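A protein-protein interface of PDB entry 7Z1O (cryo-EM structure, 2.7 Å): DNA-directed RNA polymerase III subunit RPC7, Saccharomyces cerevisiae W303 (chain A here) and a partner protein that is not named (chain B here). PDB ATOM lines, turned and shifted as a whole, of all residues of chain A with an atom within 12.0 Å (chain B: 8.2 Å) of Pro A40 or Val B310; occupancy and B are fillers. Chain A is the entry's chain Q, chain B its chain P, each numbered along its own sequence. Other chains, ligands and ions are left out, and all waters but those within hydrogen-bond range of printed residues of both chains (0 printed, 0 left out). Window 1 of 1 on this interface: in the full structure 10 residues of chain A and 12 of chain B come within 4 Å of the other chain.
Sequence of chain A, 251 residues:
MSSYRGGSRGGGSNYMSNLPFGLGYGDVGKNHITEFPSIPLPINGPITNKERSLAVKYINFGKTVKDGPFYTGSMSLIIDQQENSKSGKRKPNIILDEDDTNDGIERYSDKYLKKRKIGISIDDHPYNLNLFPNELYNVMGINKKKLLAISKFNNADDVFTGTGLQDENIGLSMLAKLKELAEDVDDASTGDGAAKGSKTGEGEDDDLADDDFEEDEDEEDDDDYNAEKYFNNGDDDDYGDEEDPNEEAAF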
ATOM      1  N   PHE A  36     -13.600   8.239  -0.082  1.00  0.00           N
ATOM      2  CA  PHE A  36     -14.160   8.889   1.084  1.00  0.00           C
ATOM      3  C   PHE A  36     -14.933   7.891   1.938  1.00  0.00           C
ATOM      4  O   PHE A  36     -15.795   7.172   1.423  1.00  0.00           O
ATOM      5  CB  PHE A  36     -15.087  10.040   0.672  1.00  0.00           C
ATOM      6  CG  PHE A  36     -14.419  11.080  -0.180  1.00  0.00           C
ATOM      7  CD1 PHE A  36     -13.763  12.152   0.399  1.00  0.00           C
ATOM      8  CD2 PHE A  36     -14.447  10.986  -1.562  1.00  0.00           C
ATOM      9  CE1 PHE A  36     -13.146  13.108  -0.381  1.00  0.00           C
ATOM     10  CE2 PHE A  36     -13.832  11.939  -2.347  1.00  0.00           C
ATOM     11  CZ  PHE A  36     -13.182  13.002  -1.756  1.00  0.00           C
ATOM     12  N   PRO A  37     -14.647   7.824   3.234  1.00  0.00           N
ATOM     13  CA  PRO A  37     -15.337   6.863   4.099  1.00  0.00           C
ATOM     14  C   PRO A  37     -16.782   7.262   4.356  1.00  0.00           C
ATOM     15  O   PRO A  37     -17.184   8.414   4.187  1.00  0.00           O
ATOM     16  CB  PRO A  37     -14.515   6.898   5.388  1.00  0.00           C
ATOM     17  CG  PRO A  37     -13.902   8.256   5.391  1.00  0.00           C
ATOM     18  CD  PRO A  37     -13.617   8.583   3.961  1.00  0.00           C
ATOM     19  N   SER A  38     -17.575   6.269   4.779  1.00  0.00           N
ATOM     20  CA  SER A  38     -18.992   6.497   5.034  1.00  0.00           C
ATOM     21  C   SER A  38     -19.483   5.816   6.309  1.00  0.00           C
ATOM     22  O   SER A  38     -20.697   5.669   6.490  1.00  0.00           O
ATOM     23  CB  SER A  38     -19.835   6.022   3.848  1.00  0.00           C
ATOM     24  OG  SER A  38     -19.507   6.738   2.669  1.00  0.00           O
ATOM     25  N   ILE A  39     -18.584   5.399   7.196  1.00  0.00           N
ATOM     26  CA  ILE A  39     -18.971   4.724   8.435  1.00  0.00           C
ATOM     27  C   ILE A  39     -18.476   5.543   9.621  1.00  0.00           C
ATOM     28  O   ILE A  39     -17.313   5.403  10.025  1.00  0.00           O
ATOM     29  CB  ILE A  39     -18.422   3.291   8.487  1.00  0.00           C
ATOM     30  CG1 ILE A  39     -18.749   2.542   7.196  1.00  0.00           C
ATOM     31  CG2 ILE A  39     -18.992   2.551   9.677  1.00  0.00           C
ATOM     32  CD1 ILE A  39     -18.234   1.125   7.168  1.00  0.00           C
ATOM     33  N   PRO A  40     -19.306   6.401  10.205  1.00  0.00           N
ATOM     34  CA  PRO A  40     -18.837   7.252  11.299  1.00  0.00           C
ATOM     35  C   PRO A  40     -19.010   6.610  12.666  1.00  0.00           C
ATOM     36  O   PRO A  40     -19.951   5.854  12.919  1.00  0.00           O
ATOM     37  CB  PRO A  40     -19.720   8.497  11.166  1.00  0.00           C
ATOM     38  CG  PRO A  40     -21.000   7.967  10.622  1.00  0.00           C
ATOM     39  CD  PRO A  40     -20.661   6.770   9.763  1.00  0.00           C
ATOM     40  N   LEU A  41     -18.071   6.924  13.553  1.00  0.00           N
ATOM     41  CA  LEU A  41     -18.169   6.559  14.954  1.00  0.00           C
ATOM     42  C   LEU A  41     -19.213   7.433  15.646  1.00  0.00           C
ATOM     43  O   LEU A  41     -19.497   8.547  15.196  1.00  0.00           O
ATOM     44  CB  LEU A  41     -16.807   6.717  15.626  1.00  0.00           C
ATOM     45  CG  LEU A  41     -15.837   5.535  15.538  1.00  0.00           C
ATOM     46  CD1 LEU A  41     -14.442   5.955  15.960  1.00  0.00           C
ATOM     47  CD2 LEU A  41     -16.320   4.369  16.378  1.00  0.00           C
ATOM     48  N   PRO A  42     -19.807   6.959  16.745  1.00  0.00           N
ATOM     49  CA  PRO A  42     -20.798   7.774  17.462  1.00  0.00           C
ATOM     50  C   PRO A  42     -20.204   8.916  18.269  1.00  0.00           C
ATOM     51  O   PRO A  42     -20.954   9.621  18.955  1.00  0.00           O
ATOM     52  CB  PRO A  42     -21.482   6.761  18.395  1.00  0.00           C
ATOM     53  CG  PRO A  42     -21.000   5.431  17.984  1.00  0.00           C
ATOM     54  CD  PRO A  42     -19.685   5.618  17.336  1.00  0.00           C
ATOM     55  N   ILE A  43     -18.887   9.120  18.208  1.00  0.00           N
ATOM     56  CA  ILE A  43     -18.230  10.163  18.990  1.00  0.00           C
ATOM     57  C   ILE A  43     -18.426  11.558  18.423  1.00  0.00           C
ATOM     58  O   ILE A  43     -17.915  12.525  19.000  1.00  0.00           O
ATOM     59  CB  ILE A  43     -16.722   9.871  19.079  1.00  0.00           C
ATOM     60  CG1 ILE A  43     -16.117   9.890  17.680  1.00  0.00           C
ATOM     61  CG2 ILE A  43     -16.480   8.522  19.725  1.00  0.00           C
ATOM     62  CD1 ILE A  43     -14.636   9.758  17.671  1.00  0.00           C
ATOM     63  N   ASN A  44     -19.147  11.696  17.310  1.00  0.00           N
ATOM     64  CA  ASN A  44     -19.293  12.975  16.625  1.00  0.00           C
ATOM     65  C   ASN A  44     -20.534  13.742  17.058  1.00  0.00           C
ATOM     66  O   ASN A  44     -21.048  14.565  16.290  1.00  0.00           O
ATOM     67  CB  ASN A  44     -19.303  12.755  15.115  1.00  0.00           C
ATOM     68  CG  ASN A  44     -18.316  11.701  14.676  1.00  0.00           C
ATOM     69  OD1 ASN A  44     -17.129  11.781  14.987  1.00  0.00           O
ATOM     70  ND2 ASN A  44     -18.799  10.705  13.947  1.00  0.00           N
ATOM     71  N   GLY A  45     -21.030  13.503  18.269  1.00  0.00           N
ATOM     72  CA  GLY A  45     -22.204  14.191  18.745  1.00  0.00           C
ATOM     73  C   GLY A  45     -21.892  15.594  19.217  1.00  0.00           C
ATOM     74  O   GLY A  45     -20.747  16.062  19.191  1.00  0.00           O
ATOM     75  N   PRO A  46     -22.939  16.297  19.647  1.00  0.00           N
ATOM     76  CA  PRO A  46     -22.748  17.653  20.174  1.00  0.00           C
ATOM     77  C   PRO A  46     -21.970  17.642  21.481  1.00  0.00           C
ATOM     78  O   PRO A  46     -22.022  16.684  22.256  1.00  0.00           O
ATOM     79  CB  PRO A  46     -24.179  18.164  20.381  1.00  0.00           C
ATOM     80  CG  PRO A  46     -25.048  17.246  19.578  1.00  0.00           C
ATOM     81  CD  PRO A  46     -24.361  15.923  19.589  1.00  0.00           C
ATOM     82  N   PRO B 301     -25.961  11.900  15.127  1.00  0.00           N
ATOM     83  CA  PRO B 301     -24.966  12.039  14.059  1.00  0.00           C
ATOM     84  C   PRO B 301     -24.528  13.485  13.881  1.00  0.00           C
ATOM     85  O   PRO B 301     -25.261  14.426  14.196  1.00  0.00           O
ATOM     86  CB  PRO B 301     -25.699  11.526  12.814  1.00  0.00           C
ATOM     87  CG  PRO B 301     -26.878  10.764  13.334  1.00  0.00           C
ATOM     88  CD  PRO B 301     -27.255  11.427  14.615  1.00  0.00           C
ATOM     89  N   ALA B 302     -23.311  13.648  13.374  1.00  0.00           N
ATOM     90  CA  ALA B 302     -22.762  14.977  13.150  1.00  0.00           C
ATOM     91  C   ALA B 302     -23.469  15.669  11.991  1.00  0.00           C
ATOM     92  O   ALA B 302     -23.950  15.029  11.053  1.00  0.00           O
ATOM     93  CB  ALA B 302     -21.263  14.897  12.867  1.00  0.00           C
ATOM     94  N   ASP B 306     -19.113  19.202   8.097  1.00  0.00           N
ATOM     95  CA  ASP B 306     -18.221  19.144   9.247  1.00  0.00           C
ATOM     96  C   ASP B 306     -16.964  18.390   8.835  1.00  0.00           C
ATOM     97  O   ASP B 306     -17.019  17.184   8.569  1.00  0.00           O
ATOM     98  CB  ASP B 306     -18.898  18.464  10.437  1.00  0.00           C
ATOM     99  CG  ASP B 306     -18.287  18.867  11.764  1.00  0.00           C
ATOM    100  OD1 ASP B 306     -17.453  19.796  11.779  1.00  0.00           O
ATOM    101  OD2 ASP B 306     -18.646  18.260  12.794  1.00  0.00           O
ATOM    102  N   LYS B 307     -15.838  19.103   8.780  1.00  0.00           N
ATOM    103  CA  LYS B 307     -14.605  18.502   8.284  1.00  0.00           C
ATOM    104  C   LYS B 307     -13.999  17.545   9.305  1.00  0.00           C
ATOM    105  O   LYS B 307     -13.475  16.487   8.938  1.00  0.00           O
ATOM    106  CB  LYS B 307     -13.601  19.594   7.918  1.00  0.00           C
ATOM    107  CG  LYS B 307     -13.848  20.248   6.568  1.00  0.00           C
ATOM    108  CD  LYS B 307     -14.715  21.488   6.711  1.00  0.00           C
ATOM    109  CE  LYS B 307     -14.707  22.323   5.441  1.00  0.00           C
ATOM    110  NZ  LYS B 307     -15.529  23.556   5.591  1.00  0.00           N
ATOM    111  N   GLU B 308     -14.062  17.898  10.587  1.00  0.00           N
ATOM    112  CA  GLU B 308     -13.359  17.162  11.638  1.00  0.00           C
ATOM    113  C   GLU B 308     -14.278  16.099  12.260  1.00  0.00           C
ATOM    114  O   GLU B 308     -14.552  16.049  13.461  1.00  0.00           O
ATOM    115  CB  GLU B 308     -12.776  18.152  12.648  1.00  0.00           C
ATOM    116  CG  GLU B 308     -13.773  18.927  13.515  1.00  0.00           C
ATOM    117  CD  GLU B 308     -14.314  20.172  12.851  1.00  0.00           C
ATOM    118  OE1 GLU B 308     -14.170  20.316  11.618  1.00  0.00           O
ATOM    119  OE2 GLU B 308     -14.908  20.999  13.569  1.00  0.00           O
ATOM    120  N   VAL B 309     -14.700  15.177  11.403  1.00  0.00           N
ATOM    121  CA  VAL B 309     -15.573  14.075  11.789  1.00  0.00           C
ATOM    122  C   VAL B 309     -14.797  12.770  11.630  1.00  0.00           C
ATOM    123  O   VAL B 309     -14.061  12.590  10.652  1.00  0.00           O
ATOM    124  CB  VAL B 309     -16.887  14.088  10.980  1.00  0.00           C
ATOM    125  CG1 VAL B 309     -16.638  13.906   9.497  1.00  0.00           C
ATOM    126  CG2 VAL B 309     -17.836  13.017  11.481  1.00  0.00           C
ATOM    127  N   VAL B 310     -14.914  11.893  12.624  1.00  0.00           N
ATOM    128  CA  VAL B 310     -14.080  10.699  12.716  1.00  0.00           C
ATOM    129  C   VAL B 310     -14.820   9.517  12.107  1.00  0.00           C
ATOM    130  O   VAL B 310     -15.955   9.215  12.492  1.00  0.00           O
ATOM    131  CB  VAL B 310     -13.695  10.414  14.176  1.00  0.00           C
ATOM    132  CG1 VAL B 310     -12.924   9.109  14.278  1.00  0.00           C
ATOM    133  CG2 VAL B 310     -12.882  11.560  14.742  1.00  0.00           C
ATOM    134  N   TYR B 311     -14.171   8.840  11.164  1.00  0.00           N
ATOM    135  CA  TYR B 311     -14.753   7.710  10.452  1.00  0.00           C
ATOM    136  C   TYR B 311     -14.014   6.431  10.817  1.00  0.00           C
ATOM    137  O   TYR B 311     -12.781   6.417  10.885  1.00  0.00           O
ATOM    138  CB  TYR B 311     -14.692   7.923   8.941  1.00  0.00           C
ATOM    139  CG  TYR B 311     -15.722   8.881   8.399  1.00  0.00           C
ATOM    140  CD1 TYR B 311     -17.046   8.496   8.249  1.00  0.00           C
ATOM    141  CD2 TYR B 311     -15.369  10.167   8.022  1.00  0.00           C
ATOM    142  CE1 TYR B 311     -17.990   9.368   7.749  1.00  0.00           C
ATOM    143  CE2 TYR B 311     -16.302  11.040   7.517  1.00  0.00           C
ATOM    144  CZ  TYR B 311     -17.612  10.640   7.386  1.00  0.00           C
ATOM    145  OH  TYR B 311     -18.545  11.515   6.885  1.00  0.00           O
ATOM    146  N   PHE B 312     -14.774   5.361  11.047  1.00  0.00           N
ATOM    147  CA  PHE B 312     -14.167   4.059  11.296  1.00  0.00           C
ATOM    148  C   PHE B 312     -13.638   3.435  10.011  1.00  0.00           C
ATOM    149  O   PHE B 312     -12.680   2.654  10.051  1.00  0.00           O
ATOM    150  CB  PHE B 312     -15.185   3.135  11.961  1.00  0.00           C
ATOM    151  CG  PHE B 312     -14.613   1.826  12.417  1.00  0.00           C
ATOM    152  CD1 PHE B 312     -13.749   1.773  13.496  1.00  0.00           C
ATOM    153  CD2 PHE B 312     -14.959   0.646  11.782  1.00  0.00           C
ATOM    154  CE1 PHE B 312     -13.227   0.571  13.921  1.00  0.00           C
ATOM    155  CE2 PHE B 312     -14.441  -0.559  12.205  1.00  0.00           C
ATOM    156  CZ  PHE B 312     -13.574  -0.597  13.275  1.00  0.00           C
ATOM    157  N   ASP B 313     -14.241   3.767   8.869  1.00  0.00           N
ATOM    158  CA  ASP B 313     -13.816   3.181   7.603  1.00  0.00           C
ATOM    159  C   ASP B 313     -12.507   3.797   7.122  1.00  0.00           C
ATOM    160  O   ASP B 313     -11.804   3.209   6.293  1.00  0.00           O
ATOM    161  CB  ASP B 313     -14.915   3.362   6.555  1.00  0.00           C
ATOM    162  CG  ASP B 313     -14.738   2.453   5.352  1.00  0.00           C
ATOM    163  OD1 ASP B 313     -13.882   1.545   5.401  1.00  0.00           O
ATOM    164  OD2 ASP B 313     -15.460   2.649   4.351  1.00  0.00           O
ATOM    165  N   GLU B 314     -12.165   4.978   7.631  1.00  0.00           N
ATOM    166  CA  GLU B 314     -10.935   5.644   7.228  1.00  0.00           C
ATOM    167  C   GLU B 314      -9.729   4.872   7.753  1.00  0.00           C
ATOM    168  O   GLU B 314      -9.841   4.068   8.684  1.00  0.00           O
ATOM    169  CB  GLU B 314     -10.928   7.084   7.739  1.00  0.00           C
ATOM    170  CG  GLU B 314     -10.144   8.056   6.880  1.00  0.00           C
ATOM    171  CD  GLU B 314     -10.480   9.502   7.189  1.00  0.00           C
ATOM    172  OE1 GLU B 314     -11.235   9.746   8.153  1.00  0.00           O
ATOM    173  OE2 GLU B 314      -9.995  10.395   6.467  1.00  0.00           O
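The backbone carbonyl oxygen (O) of Val B310 is in hydrogen-bond range of the backbone NH (N) of Leu A41 (3.3 Å).
The backbone NH of Val B310 lies within hydrogen-bond range of the side-chain amide oxygen of Asn A44 (3.2 Å).
The backbone carbonyl oxygen (O) of Ile A39 lies within hydrogen-bond range of the backbone NH (N) of Phe B312, at 2.7 Å.
ND2 of Asn A44 sits at hydrogen-bond distance from O of Leu A41 (2.6 Å).
Among the printed residues, pairs that only touch across the chains: Asn A44 with Ala B302 (3.4 Å), Ile A39 with Tyr B311 (3.5 Å), Asn A44 with Val B309 (3.5 Å), Pro A37 with Tyr B311 (3.6 Å), Pro A40 with Tyr B311 (3.7 Å), Ile A39 with Asp B313 (3.7 Å), Ile A43 with Val B310 (3.7 Å), Pro A40 with Val B310 (3.7 Å), Pro A37 with Asp B313 (3.7 Å) and Pro A37 with Glu B314 (3.8 Å).
Of the printed residues of chain B, Pro A37 touches Tyr B311 (3.6 Å), Asp B313 (3.7 Å) and Glu B314 (3.8 Å).
Printed residues of chain B within 4 Å of Ile A39: Tyr B311 (3.5 Å), Phe B312 (2.7 Å) and Asp B313 (3.7 Å).
Of chain B, only Val B310 and Tyr B311 come within 4 Å of Pro A40.
Printed residues of chain B within 4 Å of Asn A44: Ala B302, Val B309 and Val B310.
Glu B308 touches none of the printed residues of chain A.
Of chain A, only Asn A44 comes within 4 Å of Val B309.
Of chain A, only Pro A40 (3.7 Å), Leu A41 (3.3 Å), Ile A43 (3.7 Å) and Asn A44 (3.2 Å) come within 4 Å of Val B310.
Of chain A, only Pro A37, Ile A39 and Pro A40 come within 4 Å of Tyr B311.
Of the printed residues of chain A, Phe B312 touches Ile A39 (2.7 Å).
Of the printed residues of chain A, Asp B313 touches Pro A37 and Ile A39.
The nearest residue of chain B that does not touch Pro A40 is Phe B312 (4.5 Å).
The nearest residue of chain A that does not touch Val B310 is Ile A39 (4.7 Å).
Of the 11 printed residues of chain B, 7 touch a printed residue of chain A.
Hydrophobic or aromatic side chains of chain B within 4 Å of the printed part of chain A: Ala B302, Val B309, Val B310, Tyr B311 and Phe B312.
Among the printed residues, no Asp or Glu carboxylate lies within 4 Å of a Lys or Arg side-chain nitrogen of the other chain.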
